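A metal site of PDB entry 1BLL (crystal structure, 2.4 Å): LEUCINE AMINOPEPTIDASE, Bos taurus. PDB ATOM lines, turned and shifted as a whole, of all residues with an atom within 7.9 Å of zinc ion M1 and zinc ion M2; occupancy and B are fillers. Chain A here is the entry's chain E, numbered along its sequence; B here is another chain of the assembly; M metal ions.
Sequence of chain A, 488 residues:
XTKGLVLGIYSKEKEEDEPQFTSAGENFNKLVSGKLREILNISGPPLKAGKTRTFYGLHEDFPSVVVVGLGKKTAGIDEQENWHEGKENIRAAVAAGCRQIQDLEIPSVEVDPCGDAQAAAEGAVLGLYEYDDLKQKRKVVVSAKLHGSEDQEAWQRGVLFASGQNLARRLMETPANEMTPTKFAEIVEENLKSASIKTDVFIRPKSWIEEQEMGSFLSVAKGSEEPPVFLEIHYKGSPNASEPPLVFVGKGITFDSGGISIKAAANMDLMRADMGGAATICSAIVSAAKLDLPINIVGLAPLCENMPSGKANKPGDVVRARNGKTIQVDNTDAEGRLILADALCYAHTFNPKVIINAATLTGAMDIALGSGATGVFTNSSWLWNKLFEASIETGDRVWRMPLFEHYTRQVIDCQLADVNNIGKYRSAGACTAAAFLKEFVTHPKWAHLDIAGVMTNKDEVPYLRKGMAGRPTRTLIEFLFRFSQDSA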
ATOM      1  N   VAL A 220      30.269 -10.856   1.542  1.00  0.00           N
ATOM      2  CA  VAL A 220      29.603 -10.071   0.511  1.00  0.00           C
ATOM      3  C   VAL A 220      28.475  -9.247   1.099  1.00  0.00           C
ATOM      4  O   VAL A 220      28.396  -8.059   0.775  1.00  0.00           O
ATOM      5  CB  VAL A 220      29.006 -10.955  -0.573  1.00  0.00           C
ATOM      6  CG1 VAL A 220      28.422 -10.059  -1.661  1.00  0.00           C
ATOM      7  CG2 VAL A 220      30.073 -11.812  -1.240  1.00  0.00           C
ATOM      8  N   LYS A 251      21.931 -18.041  -7.166  1.00  0.00           N
ATOM      9  CA  LYS A 251      22.495 -16.781  -6.728  1.00  0.00           C
ATOM     10  C   LYS A 251      21.396 -15.757  -6.483  1.00  0.00           C
ATOM     11  O   LYS A 251      20.574 -15.504  -7.359  1.00  0.00           O
ATOM     12  CB  LYS A 251      23.466 -16.282  -7.813  1.00  0.00           C
ATOM     13  CG  LYS A 251      23.746 -14.799  -7.698  1.00  0.00           C
ATOM     14  CD  LYS A 251      25.132 -14.358  -7.989  1.00  0.00           C
ATOM     15  CE  LYS A 251      25.301 -13.978  -9.416  1.00  0.00           C
ATOM     16  NZ  LYS A 251      25.786 -12.604  -9.508  1.00  0.00           N
ATOM     17  N   ILE A 253      21.735 -12.175  -5.496  1.00  0.00           N
ATOM     18  CA  ILE A 253      22.243 -10.834  -5.193  1.00  0.00           C
ATOM     19  C   ILE A 253      21.090  -9.899  -5.555  1.00  0.00           C
ATOM     20  O   ILE A 253      20.762  -9.850  -6.746  1.00  0.00           O
ATOM     21  CB  ILE A 253      23.557 -10.553  -6.017  1.00  0.00           C
ATOM     22  CG1 ILE A 253      24.700 -11.471  -5.550  1.00  0.00           C
ATOM     23  CG2 ILE A 253      23.958  -9.115  -5.847  1.00  0.00           C
ATOM     24  CD1 ILE A 253      25.010 -11.315  -4.053  1.00  0.00           C
ATOM     25  N   PHE A 255      20.828  -6.695  -5.580  1.00  0.00           N
ATOM     26  CA  PHE A 255      21.399  -5.678  -6.424  1.00  0.00           C
ATOM     27  C   PHE A 255      22.920  -5.859  -6.398  1.00  0.00           C
ATOM     28  O   PHE A 255      23.513  -5.994  -5.335  1.00  0.00           O
ATOM     29  CB  PHE A 255      20.980  -4.282  -5.932  1.00  0.00           C
ATOM     30  CG  PHE A 255      21.403  -3.238  -6.929  1.00  0.00           C
ATOM     31  CD1 PHE A 255      20.746  -3.131  -8.147  1.00  0.00           C
ATOM     32  CD2 PHE A 255      22.584  -2.521  -6.702  1.00  0.00           C
ATOM     33  CE1 PHE A 255      21.295  -2.403  -9.179  1.00  0.00           C
ATOM     34  CE2 PHE A 255      23.139  -1.783  -7.741  1.00  0.00           C
ATOM     35  CZ  PHE A 255      22.497  -1.750  -8.980  1.00  0.00           C
ATOM     36  N   ASP A 256      23.567  -5.934  -7.580  1.00  0.00           N
ATOM     37  CA  ASP A 256      25.012  -6.004  -7.696  1.00  0.00           C
ATOM     38  C   ASP A 256      25.585  -4.662  -8.175  1.00  0.00           C
ATOM     39  O   ASP A 256      25.586  -4.330  -9.348  1.00  0.00           O
ATOM     40  CB  ASP A 256      25.407  -7.151  -8.677  1.00  0.00           C
ATOM     41  CG  ASP A 256      26.906  -7.520  -8.801  1.00  0.00           C
ATOM     42  OD1 ASP A 256      27.659  -6.965  -7.966  1.00  0.00           O
ATOM     43  OD2 ASP A 256      27.289  -8.343  -9.680  1.00  0.00           O
ATOM     44  N   SER A 257      26.068  -3.795  -7.287  1.00  0.00           N
ATOM     45  CA  SER A 257      26.767  -2.569  -7.670  1.00  0.00           C
ATOM     46  C   SER A 257      28.248  -2.846  -7.870  1.00  0.00           C
ATOM     47  O   SER A 257      28.996  -1.974  -8.299  1.00  0.00           O
ATOM     48  CB  SER A 257      26.668  -1.494  -6.588  1.00  0.00           C
ATOM     49  OG  SER A 257      27.493  -1.779  -5.476  1.00  0.00           O
ATOM     50  N   GLY A 258      28.715  -4.045  -7.514  1.00  0.00           N
ATOM     51  CA  GLY A 258      30.096  -4.388  -7.596  1.00  0.00           C
ATOM     52  C   GLY A 258      30.755  -4.210  -6.262  1.00  0.00           C
ATOM     53  O   GLY A 258      31.716  -4.916  -5.983  1.00  0.00           O
ATOM     54  N   GLY A 259      30.284  -3.283  -5.411  1.00  0.00           N
ATOM     55  CA  GLY A 259      30.918  -3.004  -4.124  1.00  0.00           C
ATOM     56  C   GLY A 259      32.084  -2.072  -4.320  1.00  0.00           C
ATOM     57  O   GLY A 259      31.982  -1.128  -5.087  1.00  0.00           O
ATOM     58  N   SER A 261      34.825  -2.827  -5.863  1.00  0.00           N
ATOM     59  CA  SER A 261      35.216  -2.970  -7.268  1.00  0.00           C
ATOM     60  C   SER A 261      33.969  -2.588  -8.056  1.00  0.00           C
ATOM     61  O   SER A 261      33.346  -3.390  -8.779  1.00  0.00           O
ATOM     62  CB  SER A 261      35.605  -4.398  -7.590  1.00  0.00           C
ATOM     63  OG  SER A 261      36.706  -4.785  -6.774  1.00  0.00           O
ATOM     64  N   LYS A 263      30.953  -0.869 -10.132  1.00  0.00           N
ATOM     65  CA  LYS A 263      30.510  -0.882 -11.500  1.00  0.00           C
ATOM     66  C   LYS A 263      30.341   0.490 -12.128  1.00  0.00           C
ATOM     67  O   LYS A 263      30.093   1.479 -11.455  1.00  0.00           O
ATOM     68  CB  LYS A 263      29.172  -1.592 -11.627  1.00  0.00           C
ATOM     69  CG  LYS A 263      29.235  -3.067 -11.445  1.00  0.00           C
ATOM     70  CD  LYS A 263      27.827  -3.588 -11.631  1.00  0.00           C
ATOM     71  CE  LYS A 263      27.845  -5.079 -11.403  1.00  0.00           C
ATOM     72  NZ  LYS A 263      28.770  -5.727 -12.307  1.00  0.00           N
ATOM     73  N   MET A 271      21.196  -4.778 -12.881  1.00  0.00           N
ATOM     74  CA  MET A 271      21.707  -5.573 -11.772  1.00  0.00           C
ATOM     75  C   MET A 271      20.710  -5.878 -10.675  1.00  0.00           C
ATOM     76  O   MET A 271      21.037  -6.701  -9.823  1.00  0.00           O
ATOM     77  CB  MET A 271      22.900  -4.918 -11.092  1.00  0.00           C
ATOM     78  CG  MET A 271      24.119  -4.787 -11.984  1.00  0.00           C
ATOM     79  SD  MET A 271      24.329  -6.170 -13.116  1.00  0.00           S
ATOM     80  CE  MET A 271      25.125  -7.301 -12.066  1.00  0.00           C
ATOM     81  N   ALA A 273      18.376  -7.592 -11.318  1.00  0.00           N
ATOM     82  CA  ALA A 273      18.086  -8.963 -11.752  1.00  0.00           C
ATOM     83  C   ALA A 273      19.204  -9.948 -11.525  1.00  0.00           C
ATOM     84  O   ALA A 273      19.197 -11.026 -12.110  1.00  0.00           O
ATOM     85  CB  ALA A 273      17.796  -9.003 -13.223  1.00  0.00           C
ATOM     86  N   ASP A 274      20.151  -9.594 -10.648  1.00  0.00           N
ATOM     87  CA  ASP A 274      21.267 -10.476 -10.287  1.00  0.00           C
ATOM     88  C   ASP A 274      20.896 -11.516  -9.216  1.00  0.00           C
ATOM     89  O   ASP A 274      21.717 -12.267  -8.693  1.00  0.00           O
ATOM     90  CB  ASP A 274      22.422  -9.604  -9.813  1.00  0.00           C
ATOM     91  CG  ASP A 274      23.762 -10.225 -10.112  1.00  0.00           C
ATOM     92  OD1 ASP A 274      23.943 -10.716 -11.222  1.00  0.00           O
ATOM     93  OD2 ASP A 274      24.629 -10.213  -9.255  1.00  0.00           O
ATOM     94  N   MET A 275      19.607 -11.526  -8.839  1.00  0.00           N
ATOM     95  CA  MET A 275      18.995 -12.612  -8.070  1.00  0.00           C
ATOM     96  C   MET A 275      18.219 -13.555  -9.001  1.00  0.00           C
ATOM     97  O   MET A 275      17.392 -14.349  -8.524  1.00  0.00           O
ATOM     98  CB  MET A 275      18.026 -12.089  -6.986  1.00  0.00           C
ATOM     99  CG  MET A 275      17.164 -10.855  -7.302  1.00  0.00           C
ATOM    100  SD  MET A 275      16.217 -10.970  -8.831  1.00  0.00           S
ATOM    101  CE  MET A 275      15.088 -12.122  -8.096  1.00  0.00           C
ATOM    102  N   ASN A 306      25.092  -6.293  -2.906  1.00  0.00           N
ATOM    103  CA  ASN A 306      26.533  -6.088  -2.900  1.00  0.00           C
ATOM    104  C   ASN A 306      26.836  -4.597  -3.055  1.00  0.00           C
ATOM    105  O   ASN A 306      26.952  -4.072  -4.140  1.00  0.00           O
ATOM    106  CB  ASN A 306      27.144  -6.911  -4.034  1.00  0.00           C
ATOM    107  CG  ASN A 306      28.665  -6.879  -4.136  1.00  0.00           C
ATOM    108  OD1 ASN A 306      29.163  -6.860  -5.252  1.00  0.00           O
ATOM    109  ND2 ASN A 306      29.449  -6.921  -3.078  1.00  0.00           N
ATOM    110  N   ASN A 331      38.592  -9.199  -6.435  1.00  0.00           N
ATOM    111  CA  ASN A 331      37.640  -8.337  -7.078  1.00  0.00           C
ATOM    112  C   ASN A 331      36.340  -8.625  -6.357  1.00  0.00           C
ATOM    113  O   ASN A 331      35.858  -9.759  -6.260  1.00  0.00           O
ATOM    114  CB  ASN A 331      37.535  -8.683  -8.550  1.00  0.00           C
ATOM    115  CG  ASN A 331      36.661  -7.723  -9.339  1.00  0.00           C
ATOM    116  OD1 ASN A 331      35.512  -7.507  -9.033  1.00  0.00           O
ATOM    117  ND2 ASN A 331      37.165  -7.083 -10.393  1.00  0.00           N
ATOM    118  N   THR A 332      35.831  -7.523  -5.843  1.00  0.00           N
ATOM    119  CA  THR A 332      34.585  -7.486  -5.081  1.00  0.00           C
ATOM    120  C   THR A 332      33.308  -7.706  -5.939  1.00  0.00           C
ATOM    121  O   THR A 332      32.238  -8.017  -5.409  1.00  0.00           O
ATOM    122  CB  THR A 332      34.688  -6.140  -4.377  1.00  0.00           C
ATOM    123  OG1 THR A 332      35.673  -6.336  -3.369  1.00  0.00           O
ATOM    124  CG2 THR A 332      33.458  -5.670  -3.701  1.00  0.00           C
ATOM    125  N   ASP A 333      33.417  -7.580  -7.266  1.00  0.00           N
ATOM    126  CA  ASP A 333      32.343  -7.777  -8.225  1.00  0.00           C
ATOM    127  C   ASP A 333      32.305  -9.204  -8.758  1.00  0.00           C
ATOM    128  O   ASP A 333      31.660  -9.516  -9.772  1.00  0.00           O
ATOM    129  CB  ASP A 333      32.507  -6.760  -9.368  1.00  0.00           C
ATOM    130  CG  ASP A 333      31.305  -6.435 -10.271  1.00  0.00           C
ATOM    131  OD1 ASP A 333      30.148  -6.764  -9.916  1.00  0.00           O
ATOM    132  OD2 ASP A 333      31.516  -5.854 -11.347  1.00  0.00           O
ATOM    133  N   ALA A 334      33.019 -10.098  -8.081  1.00  0.00           N
ATOM    134  CA  ALA A 334      32.914 -11.526  -8.371  1.00  0.00           C
ATOM    135  C   ALA A 334      32.333 -12.142  -7.087  1.00  0.00           C
ATOM    136  O   ALA A 334      32.976 -12.943  -6.401  1.00  0.00           O
ATOM    137  CB  ALA A 334      34.302 -12.085  -8.679  1.00  0.00           C
ATOM    138  N   GLU A 335      31.119 -11.706  -6.729  1.00  0.00           N
ATOM    139  CA  GLU A 335      30.463 -12.053  -5.469  1.00  0.00           C
ATOM    140  C   GLU A 335      29.522 -13.203  -5.543  1.00  0.00           C
ATOM    141  O   GLU A 335      29.192 -13.861  -4.551  1.00  0.00           O
ATOM    142  CB  GLU A 335      29.678 -10.844  -4.864  1.00  0.00           C
ATOM    143  CG  GLU A 335      28.296 -10.398  -5.378  1.00  0.00           C
ATOM    144  CD  GLU A 335      28.281 -10.051  -6.858  1.00  0.00           C
ATOM    145  OE1 GLU A 335      29.198  -9.352  -7.241  1.00  0.00           O
ATOM    146  OE2 GLU A 335      27.383 -10.466  -7.590  1.00  0.00           O
ATOM    147  N   GLY A 336      29.056 -13.470  -6.753  1.00  0.00           N
ATOM    148  CA  GLY A 336      28.209 -14.633  -6.973  1.00  0.00           C
ATOM    149  C   GLY A 336      28.968 -15.877  -6.601  1.00  0.00           C
ATOM    150  O   GLY A 336      28.455 -16.668  -5.818  1.00  0.00           O
ATOM    151  N   ARG A 337      30.235 -15.934  -7.044  1.00  0.00           N
ATOM    152  CA  ARG A 337      31.197 -17.025  -6.799  1.00  0.00           C
ATOM    153  C   ARG A 337      31.208 -17.350  -5.319  1.00  0.00           C
ATOM    154  O   ARG A 337      31.064 -18.481  -4.886  1.00  0.00           O
ATOM    155  CB  ARG A 337      32.666 -16.634  -7.178  1.00  0.00           C
ATOM    156  CG  ARG A 337      33.155 -16.272  -8.611  1.00  0.00           C
ATOM    157  CD  ARG A 337      31.909 -15.877  -9.419  1.00  0.00           C
ATOM    158  NE  ARG A 337      32.009 -14.662 -10.198  1.00  0.00           N
ATOM    159  CZ  ARG A 337      31.079 -13.711 -10.235  1.00  0.00           C
ATOM    160  NH1 ARG A 337      29.963 -13.703  -9.520  1.00  0.00           N
ATOM    161  NH2 ARG A 337      31.359 -12.703 -11.032  1.00  0.00           N
ATOM    162  N   ALA A 359      22.914 -19.085 -12.127  1.00  0.00           N
ATOM    163  CA  ALA A 359      23.414 -17.776 -11.743  1.00  0.00           C
ATOM    164  C   ALA A 359      23.718 -16.824 -12.868  1.00  0.00           C
ATOM    165  O   ALA A 359      24.309 -17.211 -13.865  1.00  0.00           O
ATOM    166  CB  ALA A 359      24.716 -17.892 -10.939  1.00  0.00           C
ATOM    167  N   THR A 360      23.352 -15.550 -12.664  1.00  0.00           N
ATOM    168  CA  THR A 360      23.705 -14.458 -13.578  1.00  0.00           C
ATOM    169  C   THR A 360      25.130 -14.088 -13.158  1.00  0.00           C
ATOM    170  O   THR A 360      25.417 -13.085 -12.490  1.00  0.00           O
ATOM    171  CB  THR A 360      22.686 -13.318 -13.347  1.00  0.00           C
ATOM    172  OG1 THR A 360      22.720 -13.042 -11.962  1.00  0.00           O
ATOM    173  CG2 THR A 360      21.269 -13.682 -13.752  1.00  0.00           C
ATOM    174  N   LEU A 361      26.051 -14.986 -13.530  1.00  0.00           N
ATOM    175  CA  LEU A 361      27.408 -14.953 -13.007  1.00  0.00           C
ATOM    176  C   LEU A 361      28.464 -14.073 -13.626  1.00  0.00           C
ATOM    177  O   LEU A 361      29.235 -13.452 -12.899  1.00  0.00           O
ATOM    178  CB  LEU A 361      27.993 -16.378 -13.005  1.00  0.00           C
ATOM    179  CG  LEU A 361      28.472 -17.114 -11.755  1.00  0.00           C
ATOM    180  CD1 LEU A 361      29.838 -17.626 -12.112  1.00  0.00           C
ATOM    181  CD2 LEU A 361      28.399 -16.267 -10.505  1.00  0.00           C
ATOM    182  N   THR A 362      28.591 -14.089 -14.955  1.00  0.00           N
ATOM    183  CA  THR A 362      29.633 -13.375 -15.632  1.00  0.00           C
ATOM    184  C   THR A 362      29.061 -12.721 -16.860  1.00  0.00           C
ATOM    185  O   THR A 362      28.205 -13.279 -17.509  1.00  0.00           O
ATOM    186  CB  THR A 362      30.815 -14.346 -16.079  1.00  0.00           C
ATOM    187  OG1 THR A 362      30.377 -15.114 -17.179  1.00  0.00           O
ATOM    188  CG2 THR A 362      31.250 -15.333 -15.011  1.00  0.00           C
ATOM    189  N   L2O B   1      26.245 -10.427 -11.733  1.00  0.00           N
ATOM    190  CA  L2O B   1      27.284 -10.035 -12.679  1.00  0.00           C
ATOM    191  C2  L2O B   1      27.009 -10.882 -13.839  1.00  0.00           C
ATOM    192  C3  L2O B   1      26.757 -10.174 -15.121  1.00  0.00           C
ATOM    193  C4  L2O B   1      27.417  -8.800 -15.015  1.00  0.00           C
ATOM    194  C5  L2O B   1      25.244  -9.996 -15.326  1.00  0.00           C
ATOM    195  C6  L2O B   1      28.661 -10.265 -12.068  1.00  0.00           C
ATOM    196  O1  L2O B   1      28.648 -10.082 -10.674  1.00  0.00           O
ATOM    197  C   L2O B   1      29.684  -9.314 -12.739  1.00  0.00           C
ATOM    198  O   L2O B   1      29.497  -8.198 -13.141  1.00  0.00           O
ATOM    199  N   VAL B   2      30.891  -9.905 -12.862  1.00  0.00           N
ATOM    200  CA  VAL B   2      32.028  -9.262 -13.409  1.00  0.00           C
ATOM    201  C   VAL B   2      31.996  -9.248 -14.949  1.00  0.00           C
ATOM    202  O   VAL B   2      31.292 -10.032 -15.584  1.00  0.00           O
ATOM    203  CB  VAL B   2      33.365  -9.915 -12.969  1.00  0.00           C
ATOM    204  CG1 VAL B   2      33.545 -11.240 -13.722  1.00  0.00           C
ATOM    205  CG2 VAL B   2      34.568  -9.009 -13.260  1.00  0.00           C
ATOM    206  N   VAL B   3      32.786  -8.320 -15.529  1.00  0.00           N
ATOM    207  CA  VAL B   3      32.682  -7.969 -16.946  1.00  0.00           C
ATOM    208  C   VAL B   3      33.719  -8.649 -17.787  1.00  0.00           C
ATOM    209  O   VAL B   3      34.689  -9.110 -17.177  1.00  0.00           O
ATOM    210  CB  VAL B   3      33.144  -6.521 -17.054  1.00  0.00           C
ATOM    211  CG1 VAL B   3      32.444  -5.635 -16.015  1.00  0.00           C
ATOM    212  CG2 VAL B   3      34.636  -6.603 -16.700  1.00  0.00           C
HETATM  213 ZN    ZN M   1      29.455  -8.745  -9.330  1.00  0.00          ZN
HETATM  214 ZN    ZN M   2      26.750 -10.526  -9.702  1.00  0.00          ZN
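Five residues have an atom within 4 Å of zinc ion M2: Lys 251, Asp 256, Asp 274, Glu 335 and L2O 1 of chain B.
Along chain A the residues within 4 Å of zinc ion M2 span positions 251 to 335.
N of L2O 1 of chain B sits close to the backbone carbonyl oxygen (O) of Thr 360, at 2.9 Å.
The side-chain amino group (NZ) of Lys 263 is in hydrogen-bond range of O of L2O 1 of chain B, at 2.7 Å.
The side-chain carboxylate (OD2) of Asp 333 lies within salt-bridge range of the side-chain amino group (NZ) of Lys 263.
The guanidinium group of Arg 337 sits close to the backbone carbonyl oxygen of Asp 333, at 3.4 Å.
The side-chain amide oxygen of Asn 306 sits close to the side-chain carboxylate of Glu 335, 3.2 Å away.
OD1 of Asp 274 sits at hydrogen-bond distance from OG1 of Thr 360 (2.7 Å).
O of Asp 274 sits at hydrogen-bond distance from N of Ile 253 (3.2 Å).
The side-chain carboxylate (OD1) of Asp 256 lies close to the side-chain amide oxygen (OD1) of Asn 306 (3.1 Å).
Merely in contact with zinc ion M1: Val 2 of chain B (3.99 Å).
Five residues have an atom within 4 Å of zinc ion M1: Asp 256, Asp 333, Glu 335, L2O 1 of chain B and Val 2 of chain B.
N of L2O 1 of chain B binds zinc ion M2 (2.1 Å).
O1 of L2O 1 of chain B binds zinc ion M2.
Zinc ion M2 is bound by OD2 of Asp 274 (2.2 Å).
Zinc ion M2 is bound by OE2 of Glu 335 (2.2 Å).
The side-chain carboxylate (OD2) of Asp 256 is bound to zinc ion M2 (2.2 Å).
NZ of Lys 251 is bound to zinc ion M2, 2.3 Å away.
O1 of L2O 1 of chain B binds zinc ion M1, 2.1 Å away.
OD1 of Asp 333 binds zinc ion M1 (2.2 Å).
OE1 of Glu 335 binds zinc ion M1 (2.2 Å).
Zinc ion M1 is bound by OD2 of Asp 256, 2.2 Å away.
The backbone carbonyl oxygen (O) of Asp 333 is bound to zinc ion M1.
Zinc ion M1 has five donor atoms within binding distance.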
